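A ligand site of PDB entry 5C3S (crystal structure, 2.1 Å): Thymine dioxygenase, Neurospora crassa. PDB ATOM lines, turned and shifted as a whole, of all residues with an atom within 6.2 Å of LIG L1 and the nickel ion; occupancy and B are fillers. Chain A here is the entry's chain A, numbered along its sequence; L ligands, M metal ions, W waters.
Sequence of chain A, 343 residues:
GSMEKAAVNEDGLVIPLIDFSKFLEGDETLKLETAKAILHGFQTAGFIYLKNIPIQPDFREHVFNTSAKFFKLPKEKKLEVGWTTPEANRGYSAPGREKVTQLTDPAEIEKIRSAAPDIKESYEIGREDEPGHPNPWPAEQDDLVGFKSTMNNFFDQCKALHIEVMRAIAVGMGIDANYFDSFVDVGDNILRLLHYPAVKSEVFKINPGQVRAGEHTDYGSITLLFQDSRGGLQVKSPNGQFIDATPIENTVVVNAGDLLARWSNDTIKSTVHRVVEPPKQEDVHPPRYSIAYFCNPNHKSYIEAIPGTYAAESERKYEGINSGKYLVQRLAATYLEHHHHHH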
ATOM      1  N   LYS A 120       2.366   8.276  -6.247  1.00  0.00           N
ATOM      2  CA  LYS A 120       0.967   7.892  -6.268  1.00  0.00           C
ATOM      3  C   LYS A 120       0.388   8.026  -4.876  1.00  0.00           C
ATOM      4  O   LYS A 120       1.116   8.089  -3.892  1.00  0.00           O
ATOM      5  CB  LYS A 120       0.803   6.436  -6.748  1.00  0.00           C
ATOM      6  CG  LYS A 120       1.355   5.393  -5.786  1.00  0.00           C
ATOM      7  CD  LYS A 120       1.119   3.960  -6.266  1.00  0.00           C
ATOM      8  CE  LYS A 120       1.462   2.945  -5.184  1.00  0.00           C
ATOM      9  NZ  LYS A 120       0.926   1.599  -5.502  1.00  0.00           N
ATOM     10  N   ARG A 192      -9.793   0.025  -4.962  1.00  0.00           N
ATOM     11  CA  ARG A 192      -8.654   0.916  -4.801  1.00  0.00           C
ATOM     12  C   ARG A 192      -8.724   2.103  -5.749  1.00  0.00           C
ATOM     13  O   ARG A 192      -8.518   1.960  -6.961  1.00  0.00           O
ATOM     14  CB  ARG A 192      -7.343   0.160  -5.013  1.00  0.00           C
ATOM     15  CG  ARG A 192      -6.090   1.015  -4.868  1.00  0.00           C
ATOM     16  CD  ARG A 192      -4.848   0.262  -5.310  1.00  0.00           C
ATOM     17  NE  ARG A 192      -4.079  -0.256  -4.179  1.00  0.00           N
ATOM     18  CZ  ARG A 192      -2.893  -0.862  -4.277  1.00  0.00           C
ATOM     19  NH1 ARG A 192      -2.327  -1.057  -5.465  1.00  0.00           N
ATOM     20  NH2 ARG A 192      -2.281  -1.281  -3.184  1.00  0.00           N
ATOM     21  N   LEU A 194      -7.026   5.304  -7.260  1.00  0.00           N
ATOM     22  CA  LEU A 194      -5.637   5.711  -7.467  1.00  0.00           C
ATOM     23  C   LEU A 194      -5.549   7.092  -8.105  1.00  0.00           C
ATOM     24  O   LEU A 194      -6.316   7.427  -9.009  1.00  0.00           O
ATOM     25  CB  LEU A 194      -4.889   4.702  -8.337  1.00  0.00           C
ATOM     26  CG  LEU A 194      -4.455   3.429  -7.621  1.00  0.00           C
ATOM     27  CD1 LEU A 194      -4.432   2.252  -8.583  1.00  0.00           C
ATOM     28  CD2 LEU A 194      -3.100   3.619  -6.967  1.00  0.00           C
ATOM     29  N   TYR A 196      -2.326   9.459  -9.488  1.00  0.00           N
ATOM     30  CA  TYR A 196      -0.915   9.671  -9.755  1.00  0.00           C
ATOM     31  C   TYR A 196      -0.765  11.166 -10.053  1.00  0.00           C
ATOM     32  O   TYR A 196      -1.169  11.604 -11.125  1.00  0.00           O
ATOM     33  CB  TYR A 196      -0.477   8.826 -10.958  1.00  0.00           C
ATOM     34  CG  TYR A 196      -0.665   7.331 -10.793  1.00  0.00           C
ATOM     35  CD1 TYR A 196      -1.871   6.712 -11.154  1.00  0.00           C
ATOM     36  CD2 TYR A 196       0.348   6.539 -10.269  1.00  0.00           C
ATOM     37  CE1 TYR A 196      -2.048   5.335 -10.995  1.00  0.00           C
ATOM     38  CE2 TYR A 196       0.178   5.168 -10.106  1.00  0.00           C
ATOM     39  CZ  TYR A 196      -1.011   4.569 -10.476  1.00  0.00           C
ATOM     40  OH  TYR A 196      -1.159   3.208 -10.313  1.00  0.00           O
ATOM     41  N   ALA A 213       3.963   3.271 -10.537  1.00  0.00           N
ATOM     42  CA  ALA A 213       3.679   2.075  -9.713  1.00  0.00           C
ATOM     43  C   ALA A 213       4.642   0.961 -10.065  1.00  0.00           C
ATOM     44  O   ALA A 213       4.745   0.593 -11.228  1.00  0.00           O
ATOM     45  CB  ALA A 213       2.250   1.613  -9.896  1.00  0.00           C
ATOM     46  N   HIS A 216       4.664  -5.681 -10.342  1.00  0.00           N
ATOM     47  CA  HIS A 216       4.038  -6.579  -9.384  1.00  0.00           C
ATOM     48  C   HIS A 216       3.067  -7.488 -10.106  1.00  0.00           C
ATOM     49  O   HIS A 216       2.770  -7.281 -11.285  1.00  0.00           O
ATOM     50  CB  HIS A 216       3.273  -5.785  -8.326  1.00  0.00           C
ATOM     51  CG  HIS A 216       2.110  -5.021  -8.892  1.00  0.00           C
ATOM     52  ND1 HIS A 216       2.265  -3.832  -9.566  1.00  0.00           N
ATOM     53  CD2 HIS A 216       0.788  -5.276  -8.895  1.00  0.00           C
ATOM     54  CE1 HIS A 216       1.095  -3.390  -9.961  1.00  0.00           C
ATOM     55  NE2 HIS A 216       0.179  -4.261  -9.573  1.00  0.00           N
ATOM     56  N   THR A 217       2.582  -8.493  -9.396  1.00  0.00           N
ATOM     57  CA  THR A 217       1.436  -9.264  -9.822  1.00  0.00           C
ATOM     58  C   THR A 217       0.339  -8.985  -8.805  1.00  0.00           C
ATOM     59  O   THR A 217       0.634  -8.745  -7.627  1.00  0.00           O
ATOM     60  CB  THR A 217       1.720 -10.789  -9.826  1.00  0.00           C
ATOM     61  OG1 THR A 217       2.245 -11.187  -8.548  1.00  0.00           O
ATOM     62  CG2 THR A 217       2.708 -11.170 -10.902  1.00  0.00           C
ATOM     63  N   ASP A 218      -0.909  -8.984  -9.253  1.00  0.00           N
ATOM     64  CA  ASP A 218      -2.034  -8.844  -8.356  1.00  0.00           C
ATOM     65  C   ASP A 218      -2.267 -10.155  -7.618  1.00  0.00           C
ATOM     66  O   ASP A 218      -1.837 -11.224  -8.079  1.00  0.00           O
ATOM     67  CB  ASP A 218      -3.301  -8.418  -9.118  1.00  0.00           C
ATOM     68  CG  ASP A 218      -3.198  -7.012  -9.676  1.00  0.00           C
ATOM     69  OD1 ASP A 218      -2.201  -6.321  -9.378  1.00  0.00           O
ATOM     70  OD2 ASP A 218      -4.102  -6.588 -10.426  1.00  0.00           O
ATOM     71  N   THR A 223      -8.675  -8.648 -11.376  1.00  0.00           N
ATOM     72  CA  THR A 223      -8.681  -7.229 -11.081  1.00  0.00           C
ATOM     73  C   THR A 223      -9.361  -6.520 -12.234  1.00  0.00           C
ATOM     74  O   THR A 223      -9.041  -6.765 -13.410  1.00  0.00           O
ATOM     75  CB  THR A 223      -7.247  -6.699 -10.915  1.00  0.00           C
ATOM     76  OG1 THR A 223      -6.614  -7.378  -9.830  1.00  0.00           O
ATOM     77  CG2 THR A 223      -7.208  -5.182 -10.646  1.00  0.00           C
ATOM     78  N   LEU A 225      -9.554  -3.157 -13.953  1.00  0.00           N
ATOM     79  CA  LEU A 225      -8.798  -1.925 -13.986  1.00  0.00           C
ATOM     80  C   LEU A 225      -9.440  -0.952 -14.946  1.00  0.00           C
ATOM     81  O   LEU A 225      -9.531  -1.218 -16.144  1.00  0.00           O
ATOM     82  CB  LEU A 225      -7.321  -2.154 -14.354  1.00  0.00           C
ATOM     83  CG  LEU A 225      -6.580  -0.820 -14.217  1.00  0.00           C
ATOM     84  CD1 LEU A 225      -6.249  -0.505 -12.765  1.00  0.00           C
ATOM     85  CD2 LEU A 225      -5.328  -0.748 -15.062  1.00  0.00           C
ATOM     86  N   PHE A 226      -9.886   0.165 -14.393  1.00  0.00           N
ATOM     87  CA  PHE A 226     -10.457   1.259 -15.151  1.00  0.00           C
ATOM     88  C   PHE A 226      -9.399   2.363 -15.195  1.00  0.00           C
ATOM     89  O   PHE A 226      -9.025   2.926 -14.155  1.00  0.00           O
ATOM     90  CB  PHE A 226     -11.713   1.794 -14.455  1.00  0.00           C
ATOM     91  CG  PHE A 226     -12.779   0.755 -14.221  1.00  0.00           C
ATOM     92  CD1 PHE A 226     -12.752  -0.047 -13.098  1.00  0.00           C
ATOM     93  CD2 PHE A 226     -13.826   0.614 -15.114  1.00  0.00           C
ATOM     94  CE1 PHE A 226     -13.754  -0.970 -12.855  1.00  0.00           C
ATOM     95  CE2 PHE A 226     -14.823  -0.332 -14.890  1.00  0.00           C
ATOM     96  CZ  PHE A 226     -14.787  -1.124 -13.772  1.00  0.00           C
ATOM     97  N   GLN A 227      -8.892   2.671 -16.388  1.00  0.00           N
ATOM     98  CA  GLN A 227      -7.889   3.721 -16.524  1.00  0.00           C
ATOM     99  C   GLN A 227      -8.435   4.893 -17.344  1.00  0.00           C
ATOM    100  O   GLN A 227      -9.313   4.710 -18.185  1.00  0.00           O
ATOM    101  CB  GLN A 227      -6.599   3.186 -17.132  1.00  0.00           C
ATOM    102  CG  GLN A 227      -6.735   2.589 -18.531  1.00  0.00           C
ATOM    103  CD  GLN A 227      -5.395   2.166 -19.103  1.00  0.00           C
ATOM    104  OE1 GLN A 227      -4.347   2.681 -18.706  1.00  0.00           O
ATOM    105  NE2 GLN A 227      -5.425   1.242 -20.046  1.00  0.00           N
ATOM    106  N   LEU A 233       0.364   2.414 -18.164  1.00  0.00           N
ATOM    107  CA  LEU A 233       0.222   1.009 -17.761  1.00  0.00           C
ATOM    108  C   LEU A 233       0.996   0.143 -18.746  1.00  0.00           C
ATOM    109  O   LEU A 233       0.845   0.291 -19.952  1.00  0.00           O
ATOM    110  CB  LEU A 233      -1.251   0.579 -17.676  1.00  0.00           C
ATOM    111  CG  LEU A 233      -1.525  -0.906 -17.354  1.00  0.00           C
ATOM    112  CD1 LEU A 233      -1.127  -1.277 -15.934  1.00  0.00           C
ATOM    113  CD2 LEU A 233      -2.984  -1.247 -17.585  1.00  0.00           C
ATOM    114  N   ASN A 255      -7.364  -8.418 -15.500  1.00  0.00           N
ATOM    115  CA  ASN A 255      -6.275  -9.389 -15.370  1.00  0.00           C
ATOM    116  C   ASN A 255      -6.495 -10.420 -14.263  1.00  0.00           C
ATOM    117  O   ASN A 255      -7.102 -10.136 -13.241  1.00  0.00           O
ATOM    118  CB  ASN A 255      -4.929  -8.689 -15.194  1.00  0.00           C
ATOM    119  CG  ASN A 255      -4.831  -7.885 -13.914  1.00  0.00           C
ATOM    120  OD1 ASN A 255      -5.546  -6.896 -13.753  1.00  0.00           O
ATOM    121  ND2 ASN A 255      -3.928  -8.277 -13.028  1.00  0.00           N
ATOM    122  N   HIS A 273       2.922  -6.462 -14.263  1.00  0.00           N
ATOM    123  CA  HIS A 273       2.550  -5.176 -14.856  1.00  0.00           C
ATOM    124  C   HIS A 273       3.049  -4.026 -13.982  1.00  0.00           C
ATOM    125  O   HIS A 273       3.405  -4.226 -12.828  1.00  0.00           O
ATOM    126  CB  HIS A 273       1.033  -5.116 -15.123  1.00  0.00           C
ATOM    127  CG  HIS A 273       0.192  -5.407 -13.916  1.00  0.00           C
ATOM    128  ND1 HIS A 273       0.045  -6.678 -13.407  1.00  0.00           N
ATOM    129  CD2 HIS A 273      -0.561  -4.605 -13.141  1.00  0.00           C
ATOM    130  CE1 HIS A 273      -0.738  -6.638 -12.342  1.00  0.00           C
ATOM    131  NE2 HIS A 273      -1.124  -5.390 -12.165  1.00  0.00           N
ATOM    132  N   ARG A 274       3.101  -2.826 -14.547  1.00  0.00           N
ATOM    133  CA  ARG A 274       3.588  -1.661 -13.814  1.00  0.00           C
ATOM    134  C   ARG A 274       2.996  -0.408 -14.437  1.00  0.00           C
ATOM    135  O   ARG A 274       2.368  -0.490 -15.490  1.00  0.00           O
ATOM    136  CB  ARG A 274       5.121  -1.603 -13.841  1.00  0.00           C
ATOM    137  CG  ARG A 274       5.692  -1.417 -15.242  1.00  0.00           C
ATOM    138  CD  ARG A 274       7.209  -1.272 -15.261  1.00  0.00           C
ATOM    139  NE  ARG A 274       7.642  -0.943 -16.610  1.00  0.00           N
ATOM    140  CZ  ARG A 274       8.908  -0.820 -16.997  1.00  0.00           C
ATOM    141  NH1 ARG A 274       9.902  -1.005 -16.137  1.00  0.00           N
ATOM    142  NH2 ARG A 274       9.170  -0.509 -18.257  1.00  0.00           N
ATOM    143  N   VAL A 275       3.194   0.744 -13.802  1.00  0.00           N
ATOM    144  CA  VAL A 275       2.862   2.029 -14.406  1.00  0.00           C
ATOM    145  C   VAL A 275       4.096   2.910 -14.457  1.00  0.00           C
ATOM    146  O   VAL A 275       4.727   3.175 -13.430  1.00  0.00           O
ATOM    147  CB  VAL A 275       1.724   2.767 -13.675  1.00  0.00           C
ATOM    148  CG1 VAL A 275       1.312   4.024 -14.446  1.00  0.00           C
ATOM    149  CG2 VAL A 275       0.512   1.870 -13.492  1.00  0.00           C
ATOM    150  N   ARG A 288      -2.770  11.438 -13.450  1.00  0.00           N
ATOM    151  CA  ARG A 288      -3.366  10.208 -13.972  1.00  0.00           C
ATOM    152  C   ARG A 288      -4.287   9.572 -12.915  1.00  0.00           C
ATOM    153  O   ARG A 288      -3.897   9.425 -11.753  1.00  0.00           O
ATOM    154  CB  ARG A 288      -2.263   9.225 -14.400  1.00  0.00           C
ATOM    155  CG  ARG A 288      -2.768   7.826 -14.730  1.00  0.00           C
ATOM    156  CD  ARG A 288      -1.726   6.965 -15.437  1.00  0.00           C
ATOM    157  NE  ARG A 288      -2.351   5.748 -15.962  1.00  0.00           N
ATOM    158  CZ  ARG A 288      -2.597   4.648 -15.245  1.00  0.00           C
ATOM    159  NH1 ARG A 288      -2.239   4.575 -13.963  1.00  0.00           N
ATOM    160  NH2 ARG A 288      -3.180   3.603 -15.812  1.00  0.00           N
ATOM    161  N   SER A 290      -6.751   6.193 -12.044  1.00  0.00           N
ATOM    162  CA  SER A 290      -7.259   4.863 -12.359  1.00  0.00           C
ATOM    163  C   SER A 290      -7.990   4.318 -11.134  1.00  0.00           C
ATOM    164  O   SER A 290      -7.902   4.874 -10.044  1.00  0.00           O
ATOM    165  CB  SER A 290      -6.133   3.920 -12.786  1.00  0.00           C
ATOM    166  OG  SER A 290      -5.233   3.703 -11.721  1.00  0.00           O
ATOM    167  N   ILE A 291      -8.720   3.243 -11.354  1.00  0.00           N
ATOM    168  CA  ILE A 291      -9.405   2.552 -10.275  1.00  0.00           C
ATOM    169  C   ILE A 291      -9.199   1.063 -10.475  1.00  0.00           C
ATOM    170  O   ILE A 291      -9.574   0.513 -11.510  1.00  0.00           O
ATOM    171  CB  ILE A 291     -10.924   2.841 -10.261  1.00  0.00           C
ATOM    172  CG1 ILE A 291     -11.197   4.358 -10.190  1.00  0.00           C
ATOM    173  CG2 ILE A 291     -11.576   2.134  -9.090  1.00  0.00           C
ATOM    174  CD1 ILE A 291     -12.663   4.712 -10.259  1.00  0.00           C
ATOM    175  N   ALA A 292      -8.579   0.436  -9.473  1.00  0.00           N
ATOM    176  CA  ALA A 292      -8.343  -0.992  -9.486  1.00  0.00           C
ATOM    177  C   ALA A 292      -9.304  -1.636  -8.498  1.00  0.00           C
ATOM    178  O   ALA A 292      -9.228  -1.403  -7.295  1.00  0.00           O
ATOM    179  CB  ALA A 292      -6.904  -1.298  -9.106  1.00  0.00           C
ATOM    180  N   PHE A 294      -9.893  -4.937  -6.973  1.00  0.00           N
ATOM    181  CA  PHE A 294      -9.310  -6.244  -6.718  1.00  0.00           C
ATOM    182  C   PHE A 294     -10.400  -7.222  -6.289  1.00  0.00           C
ATOM    183  O   PHE A 294     -11.033  -7.041  -5.259  1.00  0.00           O
ATOM    184  CB  PHE A 294      -8.251  -6.139  -5.603  1.00  0.00           C
ATOM    185  CG  PHE A 294      -7.128  -5.164  -5.914  1.00  0.00           C
ATOM    186  CD1 PHE A 294      -6.338  -5.326  -7.036  1.00  0.00           C
ATOM    187  CD2 PHE A 294      -6.866  -4.095  -5.060  1.00  0.00           C
ATOM    188  CE1 PHE A 294      -5.304  -4.439  -7.317  1.00  0.00           C
ATOM    189  CE2 PHE A 294      -5.841  -3.218  -5.337  1.00  0.00           C
ATOM    190  CZ  PHE A 294      -5.065  -3.380  -6.463  1.00  0.00           C
HETATM  191  C1  LIG L   1      -2.561  -1.883  -9.082  1.00  0.00           C
HETATM  192  O1  LIG L   1      -2.440  -3.080  -8.746  1.00  0.00           O
HETATM  193  O2  LIG L   1      -2.946  -1.020  -8.257  1.00  0.00           O
HETATM  194  C2  LIG L   1      -2.223  -1.492 -10.455  1.00  0.00           C
HETATM  195  O3  LIG L   1      -1.702  -2.313 -11.214  1.00  0.00           O
HETATM  196  C3  LIG L   1      -2.529  -0.084 -10.937  1.00  0.00           C
HETATM  197  C4  LIG L   1      -2.487  -0.008 -12.452  1.00  0.00           C
HETATM  198  C5  LIG L   1      -2.912   1.357 -12.928  1.00  0.00           C
HETATM  199  O4  LIG L   1      -3.187   1.502 -14.137  1.00  0.00           O
HETATM  200  O5  LIG L   1      -2.956   2.315 -12.115  1.00  0.00           O
HETATM  201  N1  LG2 L   2      -3.772  -4.884  -2.820  1.00  0.00           N
HETATM  202  N2  LG2 L   2      -4.708  -6.796  -3.952  1.00  0.00           N
HETATM  203  C1  LG2 L   2      -3.705  -6.689  -4.930  1.00  0.00           C
HETATM  204  C2  LG2 L   2      -2.764  -5.669  -4.818  1.00  0.00           C
HETATM  205  C3  LG2 L   2      -2.823  -4.782  -3.737  1.00  0.00           C
HETATM  206  O1  LG2 L   2      -3.678  -7.490  -5.864  1.00  0.00           O
HETATM  207  C4  LG2 L   2      -4.740  -5.892  -2.890  1.00  0.00           C
HETATM  208  O2  LG2 L   2      -5.601  -5.966  -2.026  1.00  0.00           O
HETATM  209  C5  LG2 L   2      -1.753  -5.526  -5.769  1.00  0.00           C
HETATM  210  O3  LG2 L   2      -1.478  -4.417  -6.241  1.00  0.00           O
HETATM  211 NI    NI M   1      -1.937  -4.340 -10.363  1.00  0.00          NI
HETATM  212  O   HOH W   1      -0.871   1.077  -7.956  1.00  0.00           O
HETATM  213  O   HOH W   2      -4.021  -4.336 -11.187  1.00  0.00           O
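NH2 of Arg 288 is in salt-bridge range of O4 of LIG L1, at 2.7 Å. An oxygen (O5) of LIG L1 sits at hydrogen-bond distance from the side-chain hydroxyl (OH) of Tyr 196 (2.7 Å). O5 of LIG L1 lies within hydrogen-bond range of OG of Ser 290, at 2.7 Å. An oxygen (O2) of LIG L1 lies within salt-bridge range of the guanidinium group (NH1) of Arg 192 (2.9 Å).
The side-chain amide nitrogen (ND2) of Asn 255 lies within hydrogen-bond range of the side-chain carboxylate (OD2) of Asp 218 (3.1 Å). The side-chain carboxylate of Asp 218 is in hydrogen-bond range of the side-chain hydroxyl of Thr 223 (2.7 Å). The backbone NH (N) of Tyr 196 lies within hydrogen-bond range of the backbone carbonyl oxygen (O) of Arg 288 (2.8 Å). The guanidinium group (NH2) of Arg 288 lies within hydrogen-bond range of the side-chain amide oxygen (OE1) of Gln 227 (3.3 Å). N of Leu 194 lies within hydrogen-bond range of O of Ser 290 (3.0 Å). The backbone NH (N) of Arg 192 lies within hydrogen-bond range of the backbone carbonyl oxygen (O) of Ala 292 (2.8 Å). The backbone carbonyl oxygen (O) of Val 275 sits at hydrogen-bond distance from the backbone NH (N) of Ala 213, 3.0 Å away.
Leu 194 touches LIG L1. Leu 225 touches LIG L1 (CD2 to O4, 3.2 Å). Leu 233 touches LIG L1 (CD1 to O4, 3.9 Å). Val 275 touches LIG L1. Phe 294 touches LIG L1 (CE1 to O1, 3.5 Å).
Within 4 Å of the nickel ion: His 216, Asp 218 and His 273. The nearest printed residue that does not touch the nickel ion is Phe 294 (4.5 Å).
The nickel ion is bound by O1 of LIG L1 (2.1 Å), O3 of LIG L1 (2.2 Å), OD1 of Asp 218 (2.2 Å), NE2 of His 273 (2.2 Å), water W2 (2.2 Å) and NE2 of His 216 (2.3 Å). The nickel ion has six donor atoms within binding distance.
Water W1 lies within hydrogen-bond range of O2 of LIG L1 (3.0 Å), NZ of Lys 120 (3.1 Å) and OH of Tyr 196 (3.2 Å).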
